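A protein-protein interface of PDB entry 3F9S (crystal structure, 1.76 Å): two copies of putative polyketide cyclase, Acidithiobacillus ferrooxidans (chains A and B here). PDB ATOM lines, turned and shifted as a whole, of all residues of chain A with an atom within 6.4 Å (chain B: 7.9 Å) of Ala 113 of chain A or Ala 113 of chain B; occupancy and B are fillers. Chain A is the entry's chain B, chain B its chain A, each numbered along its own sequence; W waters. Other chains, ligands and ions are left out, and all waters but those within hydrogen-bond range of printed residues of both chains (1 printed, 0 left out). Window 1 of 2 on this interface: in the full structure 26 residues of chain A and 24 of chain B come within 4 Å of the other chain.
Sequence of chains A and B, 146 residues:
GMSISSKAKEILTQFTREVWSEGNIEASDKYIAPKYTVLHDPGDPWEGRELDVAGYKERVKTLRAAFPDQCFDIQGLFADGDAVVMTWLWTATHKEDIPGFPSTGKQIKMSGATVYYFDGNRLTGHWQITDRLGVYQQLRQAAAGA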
ATOM      1  N   VAL A  85       9.376   4.814  17.615  1.00  0.00           N
ATOM      2  CA  VAL A  85       8.571   4.269  18.679  1.00  0.00           C
ATOM      3  C   VAL A  85       7.334   5.151  18.743  1.00  0.00           C
ATOM      4  O   VAL A  85       7.448   6.364  18.772  1.00  0.00           O
ATOM      5  CB  VAL A  85       9.260   4.284  20.022  1.00  0.00           C
ATOM      6  CG1 VAL A  85       8.373   3.558  21.061  1.00  0.00           C
ATOM      7  CG2 VAL A  85      10.632   3.599  19.891  1.00  0.00           C
ATOM      8  N   MET A  86       6.174   4.508  18.730  1.00  0.00           N
ATOM      9  CA  MET A  86       4.907   5.157  18.857  1.00  0.00           C
ATOM     10  C   MET A  86       4.304   4.739  20.171  1.00  0.00           C
ATOM     11  O   MET A  86       4.084   3.551  20.423  1.00  0.00           O
ATOM     12  CB  MET A  86       3.972   4.700  17.748  1.00  0.00           C
ATOM     13  CG  MET A  86       2.633   5.411  17.784  1.00  0.00           C
ATOM     14  SD  MET A  86       1.534   4.661  16.381  1.00  0.00           S
ATOM     15  CE  MET A  86       1.128   3.232  17.052  1.00  0.00           C
ATOM     16  N   THR A  87       4.022   5.719  21.007  1.00  0.00           N
ATOM     17  CA  THR A  87       3.305   5.501  22.229  1.00  0.00           C
ATOM     18  C   THR A  87       1.902   5.995  21.945  1.00  0.00           C
ATOM     19  O   THR A  87       1.698   6.943  21.179  1.00  0.00           O
ATOM     20  CB  THR A  87       3.930   6.220  23.416  1.00  0.00           C
ATOM     21  OG1 THR A  87       4.002   7.620  23.161  1.00  0.00           O
ATOM     22  CG2 THR A  87       5.351   5.660  23.660  1.00  0.00           C
ATOM     23  N   TRP A  88       0.939   5.336  22.562  1.00  0.00           N
ATOM     24  CA  TRP A  88      -0.436   5.625  22.280  1.00  0.00           C
ATOM     25  C   TRP A  88      -1.393   5.270  23.374  1.00  0.00           C
ATOM     26  O   TRP A  88      -1.111   4.400  24.193  1.00  0.00           O
ATOM     27  CB  TRP A  88      -0.879   4.892  21.000  1.00  0.00           C
ATOM     28  CG  TRP A  88      -0.470   3.479  20.914  1.00  0.00           C
ATOM     29  CD1 TRP A  88       0.671   3.016  20.347  1.00  0.00           C
ATOM     30  CD2 TRP A  88      -1.175   2.321  21.391  1.00  0.00           C
ATOM     31  NE1 TRP A  88       0.732   1.657  20.439  1.00  0.00           N
ATOM     32  CE2 TRP A  88      -0.388   1.195  21.071  1.00  0.00           C
ATOM     33  CE3 TRP A  88      -2.381   2.130  22.058  1.00  0.00           C
ATOM     34  CZ2 TRP A  88      -0.789  -0.115  21.364  1.00  0.00           C
ATOM     35  CZ3 TRP A  88      -2.788   0.826  22.362  1.00  0.00           C
ATOM     36  CH2 TRP A  88      -1.974  -0.281  22.030  1.00  0.00           C
ATOM     37  N   SER A 111      -3.446   1.459  26.500  1.00  0.00           N
ATOM     38  CA  SER A 111      -2.300   2.225  26.072  1.00  0.00           C
ATOM     39  C   SER A 111      -1.242   1.230  25.672  1.00  0.00           C
ATOM     40  O   SER A 111      -1.355   0.039  25.947  1.00  0.00           O
ATOM     41  CB  SER A 111      -1.832   3.152  27.174  1.00  0.00           C
ATOM     42  OG  SER A 111      -1.433   2.414  28.314  1.00  0.00           O
ATOM     43  N   GLY A 112      -0.271   1.709  24.929  1.00  0.00           N
ATOM     44  CA  GLY A 112       0.768   0.846  24.449  1.00  0.00           C
ATOM     45  C   GLY A 112       1.925   1.589  23.847  1.00  0.00           C
ATOM     46  O   GLY A 112       1.852   2.787  23.676  1.00  0.00           O
ATOM     47  N   ALA A 113       2.988   0.836  23.576  1.00  0.00           N
ATOM     48  CA  ALA A 113       4.193   1.381  22.960  1.00  0.00           C
ATOM     49  C   ALA A 113       4.495   0.430  21.827  1.00  0.00           C
ATOM     50  O   ALA A 113       4.493  -0.764  22.027  1.00  0.00           O
ATOM     51  CB  ALA A 113       5.341   1.418  23.948  1.00  0.00           C
ATOM     52  N   THR A 114       4.764   0.962  20.650  1.00  0.00           N
ATOM     53  CA  THR A 114       4.978   0.144  19.463  1.00  0.00           C
ATOM     54  C   THR A 114       6.191   0.682  18.737  1.00  0.00           C
ATOM     55  O   THR A 114       6.169   1.809  18.304  1.00  0.00           O
ATOM     56  CB  THR A 114       3.782   0.241  18.541  1.00  0.00           C
ATOM     57  OG1 THR A 114       2.602  -0.086  19.266  1.00  0.00           O
ATOM     58  CG2 THR A 114       3.942  -0.741  17.364  1.00  0.00           C
ATOM     59  N   VAL A 115       7.247  -0.120  18.644  1.00  0.00           N
ATOM     60  CA  VAL A 115       8.439   0.242  17.916  1.00  0.00           C
ATOM     61  C   VAL A 115       8.155  -0.227  16.509  1.00  0.00           C
ATOM     62  O   VAL A 115       7.931  -1.403  16.300  1.00  0.00           O
ATOM     63  CB  VAL A 115       9.703  -0.451  18.417  1.00  0.00           C
ATOM     64  CG1 VAL A 115      10.919   0.125  17.690  1.00  0.00           C
ATOM     65  CG2 VAL A 115       9.846  -0.245  19.948  1.00  0.00           C
ATOM     66  N   TRP A 127       7.618  -4.035  17.463  1.00  0.00           N
ATOM     67  CA  TRP A 127       7.907  -4.605  18.761  1.00  0.00           C
ATOM     68  C   TRP A 127       6.958  -3.809  19.634  1.00  0.00           C
ATOM     69  O   TRP A 127       7.123  -2.596  19.745  1.00  0.00           O
ATOM     70  CB  TRP A 127       9.344  -4.311  19.102  1.00  0.00           C
ATOM     71  CG  TRP A 127       9.903  -5.007  20.281  1.00  0.00           C
ATOM     72  CD1 TRP A 127      10.779  -6.022  20.235  1.00  0.00           C
ATOM     73  CD2 TRP A 127       9.679  -4.722  21.676  1.00  0.00           C
ATOM     74  NE1 TRP A 127      11.114  -6.415  21.494  1.00  0.00           N
ATOM     75  CE2 TRP A 127      10.482  -5.620  22.404  1.00  0.00           C
ATOM     76  CE3 TRP A 127       8.922  -3.775  22.375  1.00  0.00           C
ATOM     77  CZ2 TRP A 127      10.522  -5.642  23.812  1.00  0.00           C
ATOM     78  CZ3 TRP A 127       8.973  -3.788  23.782  1.00  0.00           C
ATOM     79  CH2 TRP A 127       9.762  -4.722  24.467  1.00  0.00           C
ATOM     80  N   GLN A 128       6.025  -4.490  20.299  1.00  0.00           N
ATOM     81  CA  GLN A 128       4.977  -3.795  20.994  1.00  0.00           C
ATOM     82  C   GLN A 128       4.662  -4.355  22.354  1.00  0.00           C
ATOM     83  O   GLN A 128       4.815  -5.543  22.593  1.00  0.00           O
ATOM     84  CB  GLN A 128       3.748  -3.875  20.119  1.00  0.00           C
ATOM     85  CG  GLN A 128       2.468  -3.349  20.707  1.00  0.00           C
ATOM     86  CD  GLN A 128       1.435  -3.288  19.666  1.00  0.00           C
ATOM     87  OE1 GLN A 128       1.320  -2.268  19.036  1.00  0.00           O
ATOM     88  NE2 GLN A 128       0.728  -4.387  19.423  1.00  0.00           N
ATOM     89  N   ILE A 129       4.206  -3.460  23.222  1.00  0.00           N
ATOM     90  CA  ILE A 129       3.731  -3.832  24.537  1.00  0.00           C
ATOM     91  C   ILE A 129       2.464  -3.014  24.706  1.00  0.00           C
ATOM     92  O   ILE A 129       2.449  -1.836  24.381  1.00  0.00           O
ATOM     93  CB  ILE A 129       4.670  -3.444  25.690  1.00  0.00           C
ATOM     94  CG1 ILE A 129       6.089  -3.952  25.516  1.00  0.00           C
ATOM     95  CG2 ILE A 129       4.124  -4.034  26.988  1.00  0.00           C
ATOM     96  CD1 ILE A 129       6.300  -5.387  25.764  1.00  0.00           C
ATOM     97  N   THR A 130       1.400  -3.650  25.167  1.00  0.00           N
ATOM     98  CA  THR A 130       0.145  -2.952  25.404  1.00  0.00           C
ATOM     99  C   THR A 130      -0.355  -3.289  26.786  1.00  0.00           C
ATOM    100  O   THR A 130       0.012  -4.331  27.353  1.00  0.00           O
ATOM    101  CB  THR A 130      -0.902  -3.354  24.404  1.00  0.00           C
ATOM    102  OG1 THR A 130      -1.344  -4.685  24.689  1.00  0.00           O
ATOM    103  CG2 THR A 130      -0.372  -3.273  22.961  1.00  0.00           C
ATOM    104  N   HIS B  40       2.953   8.106  32.820  1.00  0.00           N
ATOM    105  CA  HIS B  40       2.043   7.033  32.507  1.00  0.00           C
ATOM    106  C   HIS B  40       2.743   5.751  32.883  1.00  0.00           C
ATOM    107  O   HIS B  40       3.898   5.547  32.530  1.00  0.00           O
ATOM    108  CB  HIS B  40       1.749   7.069  31.015  1.00  0.00           C
ATOM    109  CG  HIS B  40       0.781   6.031  30.568  1.00  0.00           C
ATOM    110  ND1 HIS B  40      -0.579   6.176  30.703  1.00  0.00           N
ATOM    111  CD2 HIS B  40       0.980   4.850  29.939  1.00  0.00           C
ATOM    112  CE1 HIS B  40      -1.180   5.113  30.189  1.00  0.00           C
ATOM    113  NE2 HIS B  40      -0.254   4.278  29.752  1.00  0.00           N
ATOM    114  N   ASP B  41       2.030   4.868  33.566  1.00  0.00           N
ATOM    115  CA  ASP B  41       2.620   3.635  34.041  1.00  0.00           C
ATOM    116  C   ASP B  41       1.489   2.828  34.654  1.00  0.00           C
ATOM    117  O   ASP B  41       1.280   2.871  35.878  1.00  0.00           O
ATOM    118  CB  ASP B  41       3.705   3.923  35.083  1.00  0.00           C
ATOM    119  CG  ASP B  41       4.665   2.770  35.268  1.00  0.00           C
ATOM    120  OD1 ASP B  41       4.392   1.617  34.860  1.00  0.00           O
ATOM    121  OD2 ASP B  41       5.691   3.057  35.907  1.00  0.00           O
ATOM    122  N   PRO B  42       0.714   2.149  33.796  1.00  0.00           N
ATOM    123  CA  PRO B  42      -0.469   1.423  34.218  1.00  0.00           C
ATOM    124  C   PRO B  42      -0.306   0.626  35.490  1.00  0.00           C
ATOM    125  O   PRO B  42       0.604  -0.192  35.595  1.00  0.00           O
ATOM    126  CB  PRO B  42      -0.762   0.537  33.029  1.00  0.00           C
ATOM    127  CG  PRO B  42      -0.396   1.439  31.883  1.00  0.00           C
ATOM    128  CD  PRO B  42       0.882   2.050  32.333  1.00  0.00           C
ATOM    129  N   GLY B  76      16.318  -2.161  23.160  1.00  0.00           N
ATOM    130  CA  GLY B  76      16.556  -1.066  22.248  1.00  0.00           C
ATOM    131  C   GLY B  76      16.512   0.249  22.975  1.00  0.00           C
ATOM    132  O   GLY B  76      15.858   0.369  24.016  1.00  0.00           O
ATOM    133  N   PHE B  78      15.911   4.259  21.808  1.00  0.00           N
ATOM    134  CA  PHE B  78      15.467   5.066  20.680  1.00  0.00           C
ATOM    135  C   PHE B  78      15.411   6.503  21.169  1.00  0.00           C
ATOM    136  O   PHE B  78      14.515   6.850  21.919  1.00  0.00           O
ATOM    137  CB  PHE B  78      14.117   4.553  20.198  1.00  0.00           C
ATOM    138  CG  PHE B  78      14.112   3.086  19.962  1.00  0.00           C
ATOM    139  CD1 PHE B  78      14.505   2.562  18.739  1.00  0.00           C
ATOM    140  CD2 PHE B  78      13.741   2.209  20.987  1.00  0.00           C
ATOM    141  CE1 PHE B  78      14.511   1.174  18.533  1.00  0.00           C
ATOM    142  CE2 PHE B  78      13.770   0.845  20.780  1.00  0.00           C
ATOM    143  CZ  PHE B  78      14.141   0.332  19.560  1.00  0.00           C
ATOM    144  N   VAL B  84      14.381   9.344  25.440  1.00  0.00           N
ATOM    145  CA  VAL B  84      14.973   8.108  24.984  1.00  0.00           C
ATOM    146  C   VAL B  84      13.996   7.028  25.407  1.00  0.00           C
ATOM    147  O   VAL B  84      13.693   6.895  26.578  1.00  0.00           O
ATOM    148  CB  VAL B  84      16.349   7.814  25.536  1.00  0.00           C
ATOM    149  CG1 VAL B  84      16.885   6.503  24.913  1.00  0.00           C
ATOM    150  CG2 VAL B  84      17.305   8.985  25.218  1.00  0.00           C
ATOM    151  N   VAL B  85      13.501   6.292  24.432  1.00  0.00           N
ATOM    152  CA  VAL B  85      12.628   5.160  24.695  1.00  0.00           C
ATOM    153  C   VAL B  85      13.519   3.941  24.866  1.00  0.00           C
ATOM    154  O   VAL B  85      14.403   3.706  24.036  1.00  0.00           O
ATOM    155  CB  VAL B  85      11.645   4.897  23.572  1.00  0.00           C
ATOM    156  CG1 VAL B  85      10.693   3.749  23.999  1.00  0.00           C
ATOM    157  CG2 VAL B  85      10.817   6.145  23.216  1.00  0.00           C
ATOM    158  N   MET B  86      13.291   3.170  25.932  1.00  0.00           N
ATOM    159  CA  MET B  86      14.023   1.968  26.214  1.00  0.00           C
ATOM    160  C   MET B  86      13.015   0.836  26.155  1.00  0.00           C
ATOM    161  O   MET B  86      11.981   0.906  26.812  1.00  0.00           O
ATOM    162  CB  MET B  86      14.591   2.035  27.632  1.00  0.00           C
ATOM    163  CG  MET B  86      15.460   0.886  28.013  1.00  0.00           C
ATOM    164  SD  MET B  86      15.770   1.275  29.929  1.00  0.00           S
ATOM    165  CE  MET B  86      14.322   0.534  30.815  1.00  0.00           C
ATOM    166  N   THR B  87      13.280  -0.145  25.324  1.00  0.00           N
ATOM    167  CA  THR B  87      12.506  -1.378  25.323  1.00  0.00           C
ATOM    168  C   THR B  87      13.372  -2.334  26.097  1.00  0.00           C
ATOM    169  O   THR B  87      14.600  -2.274  26.036  1.00  0.00           O
ATOM    170  CB  THR B  87      12.203  -1.885  23.930  1.00  0.00           C
ATOM    171  OG1 THR B  87      13.404  -1.971  23.176  1.00  0.00           O
ATOM    172  CG2 THR B  87      11.225  -0.937  23.236  1.00  0.00           C
ATOM    173  N   TRP B  88      12.722  -3.249  26.815  1.00  0.00           N
ATOM    174  CA  TRP B  88      13.431  -4.143  27.691  1.00  0.00           C
ATOM    175  C   TRP B  88      12.675  -5.408  27.998  1.00  0.00           C
ATOM    176  O   TRP B  88      11.455  -5.475  27.847  1.00  0.00           O
ATOM    177  CB  TRP B  88      13.761  -3.441  29.007  1.00  0.00           C
ATOM    178  CG  TRP B  88      12.633  -2.652  29.599  1.00  0.00           C
ATOM    179  CD1 TRP B  88      12.389  -1.366  29.395  1.00  0.00           C
ATOM    180  CD2 TRP B  88      11.629  -3.119  30.501  1.00  0.00           C
ATOM    181  NE1 TRP B  88      11.281  -0.953  30.081  1.00  0.00           N
ATOM    182  CE2 TRP B  88      10.781  -2.016  30.780  1.00  0.00           C
ATOM    183  CE3 TRP B  88      11.341  -4.354  31.071  1.00  0.00           C
ATOM    184  CZ2 TRP B  88       9.704  -2.099  31.645  1.00  0.00           C
ATOM    185  CZ3 TRP B  88      10.248  -4.460  31.932  1.00  0.00           C
ATOM    186  CH2 TRP B  88       9.433  -3.329  32.204  1.00  0.00           C
ATOM    187  N   LEU B  89      13.464  -6.406  28.364  1.00  0.00           N
ATOM    188  CA  LEU B  89      12.999  -7.656  28.899  1.00  0.00           C
ATOM    189  C   LEU B  89      13.388  -7.558  30.354  1.00  0.00           C
ATOM    190  O   LEU B  89      14.228  -6.748  30.756  1.00  0.00           O
ATOM    191  CB  LEU B  89      13.702  -8.819  28.235  1.00  0.00           C
ATOM    192  CG  LEU B  89      13.485  -8.847  26.730  1.00  0.00           C
ATOM    193  CD1 LEU B  89      14.242 -10.028  26.169  1.00  0.00           C
ATOM    194  CD2 LEU B  89      12.033  -8.876  26.292  1.00  0.00           C
ATOM    195  N   SER B 111       8.288  -7.932  29.707  1.00  0.00           N
ATOM    196  CA  SER B 111       8.892  -7.012  28.761  1.00  0.00           C
ATOM    197  C   SER B 111       8.195  -5.709  28.918  1.00  0.00           C
ATOM    198  O   SER B 111       7.089  -5.640  29.439  1.00  0.00           O
ATOM    199  CB  SER B 111       8.789  -7.504  27.323  1.00  0.00           C
ATOM    200  OG  SER B 111       7.451  -7.764  26.980  1.00  0.00           O
ATOM    201  N   GLY B 112       8.871  -4.654  28.499  1.00  0.00           N
ATOM    202  CA  GLY B 112       8.285  -3.365  28.616  1.00  0.00           C
ATOM    203  C   GLY B 112       8.965  -2.355  27.739  1.00  0.00           C
ATOM    204  O   GLY B 112       9.974  -2.624  27.108  1.00  0.00           O
ATOM    205  N   ALA B 113       8.312  -1.210  27.674  1.00  0.00           N
ATOM    206  CA  ALA B 113       8.812  -0.074  26.937  1.00  0.00           C
ATOM    207  C   ALA B 113       8.638   1.134  27.829  1.00  0.00           C
ATOM    208  O   ALA B 113       7.579   1.319  28.424  1.00  0.00           O
ATOM    209  CB  ALA B 113       8.086   0.051  25.631  1.00  0.00           C
ATOM    210  N   THR B 114       9.668   1.968  27.899  1.00  0.00           N
ATOM    211  CA  THR B 114       9.656   3.104  28.773  1.00  0.00           C
ATOM    212  C   THR B 114      10.262   4.265  28.058  1.00  0.00           C
ATOM    213  O   THR B 114      11.401   4.173  27.650  1.00  0.00           O
ATOM    214  CB  THR B 114      10.501   2.815  29.984  1.00  0.00           C
ATOM    215  OG1 THR B 114      10.062   1.586  30.544  1.00  0.00           O
ATOM    216  CG2 THR B 114      10.337   3.921  31.007  1.00  0.00           C
ATOM    217  N   VAL B 115       9.473   5.310  27.890  1.00  0.00           N
ATOM    218  CA  VAL B 115       9.962   6.573  27.353  1.00  0.00           C
ATOM    219  C   VAL B 115      10.525   7.282  28.566  1.00  0.00           C
ATOM    220  O   VAL B 115       9.816   7.480  29.559  1.00  0.00           O
ATOM    221  CB  VAL B 115       8.863   7.454  26.780  1.00  0.00           C
ATOM    222  CG1 VAL B 115       9.505   8.707  26.174  1.00  0.00           C
ATOM    223  CG2 VAL B 115       8.059   6.674  25.710  1.00  0.00           C
ATOM    224  N   TYR B 116      11.781   7.679  28.480  1.00  0.00           N
ATOM    225  CA  TYR B 116      12.432   8.432  29.534  1.00  0.00           C
ATOM    226  C   TYR B 116      12.653   9.804  29.001  1.00  0.00           C
ATOM    227  O   TYR B 116      13.132   9.934  27.892  1.00  0.00           O
ATOM    228  CB  TYR B 116      13.776   7.829  29.911  1.00  0.00           C
ATOM    229  CG  TYR B 116      13.640   6.814  30.979  1.00  0.00           C
ATOM    230  CD1 TYR B 116      13.357   7.235  32.284  1.00  0.00           C
ATOM    231  CD2 TYR B 116      13.765   5.462  30.724  1.00  0.00           C
ATOM    232  CE1 TYR B 116      13.212   6.344  33.299  1.00  0.00           C
ATOM    233  CE2 TYR B 116      13.616   4.539  31.747  1.00  0.00           C
ATOM    234  CZ  TYR B 116      13.332   4.995  33.030  1.00  0.00           C
ATOM    235  OH  TYR B 116      13.198   4.136  34.081  1.00  0.00           O
ATOM    236  N   HIS B 126       8.834   9.331  33.224  1.00  0.00           N
ATOM    237  CA  HIS B 126       8.701   8.231  32.280  1.00  0.00           C
ATOM    238  C   HIS B 126       7.259   7.974  31.860  1.00  0.00           C
ATOM    239  O   HIS B 126       6.328   8.334  32.557  1.00  0.00           O
ATOM    240  CB  HIS B 126       9.359   6.949  32.776  1.00  0.00           C
ATOM    241  CG  HIS B 126       8.620   6.274  33.887  1.00  0.00           C
ATOM    242  ND1 HIS B 126       8.984   6.400  35.208  1.00  0.00           N
ATOM    243  CD2 HIS B 126       7.552   5.439  33.869  1.00  0.00           C
ATOM    244  CE1 HIS B 126       8.170   5.675  35.954  1.00  0.00           C
ATOM    245  NE2 HIS B 126       7.282   5.099  35.168  1.00  0.00           N
ATOM    246  N   TRP B 127       7.121   7.386  30.679  1.00  0.00           N
ATOM    247  CA  TRP B 127       5.859   6.961  30.116  1.00  0.00           C
ATOM    248  C   TRP B 127       6.147   5.504  29.811  1.00  0.00           C
ATOM    249  O   TRP B 127       6.976   5.196  28.960  1.00  0.00           O
ATOM    250  CB  TRP B 127       5.581   7.757  28.864  1.00  0.00           C
ATOM    251  CG  TRP B 127       4.200   7.701  28.427  1.00  0.00           C
ATOM    252  CD1 TRP B 127       3.270   8.677  28.571  1.00  0.00           C
ATOM    253  CD2 TRP B 127       3.575   6.642  27.717  1.00  0.00           C
ATOM    254  NE1 TRP B 127       2.091   8.280  28.004  1.00  0.00           N
ATOM    255  CE2 TRP B 127       2.249   7.034  27.470  1.00  0.00           C
ATOM    256  CE3 TRP B 127       4.006   5.396  27.243  1.00  0.00           C
ATOM    257  CZ2 TRP B 127       1.343   6.224  26.783  1.00  0.00           C
ATOM    258  CZ3 TRP B 127       3.096   4.590  26.572  1.00  0.00           C
ATOM    259  CH2 TRP B 127       1.779   5.005  26.358  1.00  0.00           C
ATOM    260  N   GLN B 128       5.477   4.601  30.511  1.00  0.00           N
ATOM    261  CA  GLN B 128       5.816   3.203  30.438  1.00  0.00           C
ATOM    262  C   GLN B 128       4.637   2.282  30.239  1.00  0.00           C
ATOM    263  O   GLN B 128       3.536   2.569  30.673  1.00  0.00           O
ATOM    264  CB  GLN B 128       6.496   2.839  31.748  1.00  0.00           C
ATOM    265  CG  GLN B 128       6.812   1.392  31.969  1.00  0.00           C
ATOM    266  CD  GLN B 128       7.799   1.270  33.071  1.00  0.00           C
ATOM    267  OE1 GLN B 128       8.976   1.436  32.821  1.00  0.00           O
ATOM    268  NE2 GLN B 128       7.335   1.069  34.298  1.00  0.00           N
ATOM    269  N   ILE B 129       4.890   1.198  29.524  1.00  0.00           N
ATOM    270  CA  ILE B 129       3.908   0.117  29.426  1.00  0.00           C
ATOM    271  C   ILE B 129       4.739  -1.132  29.654  1.00  0.00           C
ATOM    272  O   ILE B 129       5.827  -1.250  29.116  1.00  0.00           O
ATOM    273  CB  ILE B 129       3.230   0.037  28.043  1.00  0.00           C
ATOM    274  CG1 ILE B 129       2.672   1.382  27.619  1.00  0.00           C
ATOM    275  CG2 ILE B 129       2.138  -1.065  28.056  1.00  0.00           C
ATOM    276  CD1 ILE B 129       1.484   1.847  28.378  1.00  0.00           C
ATOM    277  N   THR B 130       4.212  -2.061  30.435  1.00  0.00           N
ATOM    278  CA  THR B 130       4.882  -3.312  30.699  1.00  0.00           C
ATOM    279  C   THR B 130       3.869  -4.427  30.508  1.00  0.00           C
ATOM    280  O   THR B 130       2.660  -4.211  30.616  1.00  0.00           O
ATOM    281  CB  THR B 130       5.390  -3.373  32.143  1.00  0.00           C
ATOM    282  OG1 THR B 130       4.281  -3.489  33.017  1.00  0.00           O
ATOM    283  CG2 THR B 130       6.165  -2.114  32.542  1.00  0.00           C
ATOM    284  N   ASP B 131       4.376  -5.628  30.278  1.00  0.00           N
ATOM    285  CA  ASP B 131       3.537  -6.804  30.085  1.00  0.00           C
ATOM    286  C   ASP B 131       3.096  -7.387  31.435  1.00  0.00           C
ATOM    287  O   ASP B 131       3.498  -8.484  31.840  1.00  0.00           O
ATOM    288  CB  ASP B 131       4.267  -7.844  29.247  1.00  0.00           C
ATOM    289  CG  ASP B 131       3.407  -9.039  28.925  1.00  0.00           C
ATOM    290  OD1 ASP B 131       2.157  -8.923  28.982  1.00  0.00           O
ATOM    291  OD2 ASP B 131       4.007 -10.081  28.603  1.00  0.00           O
HETATM  292  O   HOH W   1       0.480  -6.927  28.076  1.00  0.00           O
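Printed residues of chain A that touch a printed residue of chain B: Val 85, Thr 87, Trp 88, Ser 111, Gly 112, Ala 113, Val 115, Trp 127, Ile 129 and Thr 130. Of the 23 printed residues of chain B, 14 touch a printed residue of chain A. Printed residues of chain B that touch a printed residue of chain A: His 40, Pro 42, Phe 78, Val 85, Thr 87, Trp 88, Ser 111, Gly 112, Ala 113, Val 115, Trp 127, Ile 129, Thr 130 and Asp 131. Hydrophobic or aromatic side chains of chain B within 4 Å of the printed part of chain A: His 40, Pro 42, Phe 78, Val 85, Ala 113, Val 115, Trp 127 and Ile 129. Among the printed residues, 22 pairs touch across the chains. Among the printed residues, no Asp or Glu carboxylate lies within 4 Å of a Lys or Arg side-chain nitrogen of the other chain.
The backbone NH (N) of His 40 of chain B lies within hydrogen-bond range of the backbone carbonyl oxygen (O) of His 126 of chain B, at 3.4 Å. The side-chain hydroxyl (OG1) of Thr 87 of chain B is in hydrogen-bond range of the backbone NH (N) of Gly 76 of chain B. O of Trp 88 of chain B lies within hydrogen-bond range of N of Gly 112 of chain B. The side-chain hydroxyl (OG1) of Thr 114 of chain B is in hydrogen-bond range of the indole nitrogen (NE1) of Trp 88 of chain B, 2.9 Å away. The backbone NH of Ala 113 of chain B is in hydrogen-bond range of the backbone carbonyl oxygen of Ile 129 of chain B (2.9 Å). N of Val 115 of chain A lies within hydrogen-bond range of O of Trp 127 of chain A (2.7 Å).
Water W1 lies within hydrogen-bond range of O of Thr 130 of chain A and OD1 of Asp 131 of chain B.
Among the printed residues, pairs that only touch across the chains: Ile 129 of chain A with Ser 111 of chain B (2.9 Å), Ser 111 of chain A with Ile 129 of chain B (3.0 Å), Trp 127 of chain A with Gly 112 of chain B (3.4 Å), Gly 112 of chain A with Trp 127 of chain B (3.5 Å), Ala 113 of chain A with Ala 113 of chain B (3.5 Å), Val 85 of chain A with Phe 78 of chain B (3.5 Å), Thr 87 of chain A with Val 115 of chain B (3.5 Å), Ile 129 of chain A with Thr 130 of chain B (3.6 Å), Thr 130 of chain A with Ile 129 of chain B (3.6 Å), Val 115 of chain A with Thr 87 of chain B (3.6 Å), Thr 87 of chain A with Trp 127 of chain B (3.6 Å), Trp 88 of chain A with Trp 127 of chain B (3.7 Å), Ile 129 of chain A with Asp 131 of chain B (3.7 Å), Trp 127 of chain A with Thr 87 of chain B (3.7 Å), Ile 129 of chain A with Ile 129 of chain B (3.7 Å), Val 115 of chain A with Phe 78 of chain B (3.7 Å), Gly 112 of chain A with Ile 129 of chain B (3.7 Å), Val 85 of chain A with Val 85 of chain B (3.7 Å), Ile 129 of chain A with Gly 112 of chain B (3.8 Å), Ser 111 of chain A with Pro 42 of chain B (3.8 Å) and Trp 127 of chain A with Trp 88 of chain B (3.9 Å).
A ring nitrogen (NE2) of His 40 of chain B lies within hydrogen-bond range of the side-chain hydroxyl (OG) of Ser 111 of chain A.
Ala 113 of chain A touches just one residue of chain B: Ala 113. Gly 112 of chain A touches just these residues of chain B: Trp 127 (3.5 Å) and Ile 129 (3.7 Å). Printed residues of chain B within 4 Å of Trp 88 of chain A: Trp 127 (3.7 Å). Of the printed residues of chain A, Trp 127 of chain B touches Thr 87, Trp 88 and Gly 112. Printed residues of chain A within 4 Å of Trp 88 of chain B: Trp 127 (3.9 Å). Of the printed residues of chain A, Thr 87 of chain B touches Val 115 and Trp 127. Tyr 116 of chain B touches none of the printed residues of chain A. The nearest residue of chain B that does not touch Ala 113 of chain A is Ile 129 of chain B (4.1 Å).
Val 85 of chain B touches its own counterpart, Val 85 of chain A. Thr 87 of chain A touches Trp 127 of chain B, and with the chains exchanged Trp 127 of chain A touches Thr 87 of chain B. Ala 113 of chain B touches its own counterpart, Ala 113 of chain A. Ile 129 of chain A touches Thr 130 of chain B, and with the chains exchanged Thr 130 of chain A touches Ile 129 of chain B. 13 positions are printed for both chains.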
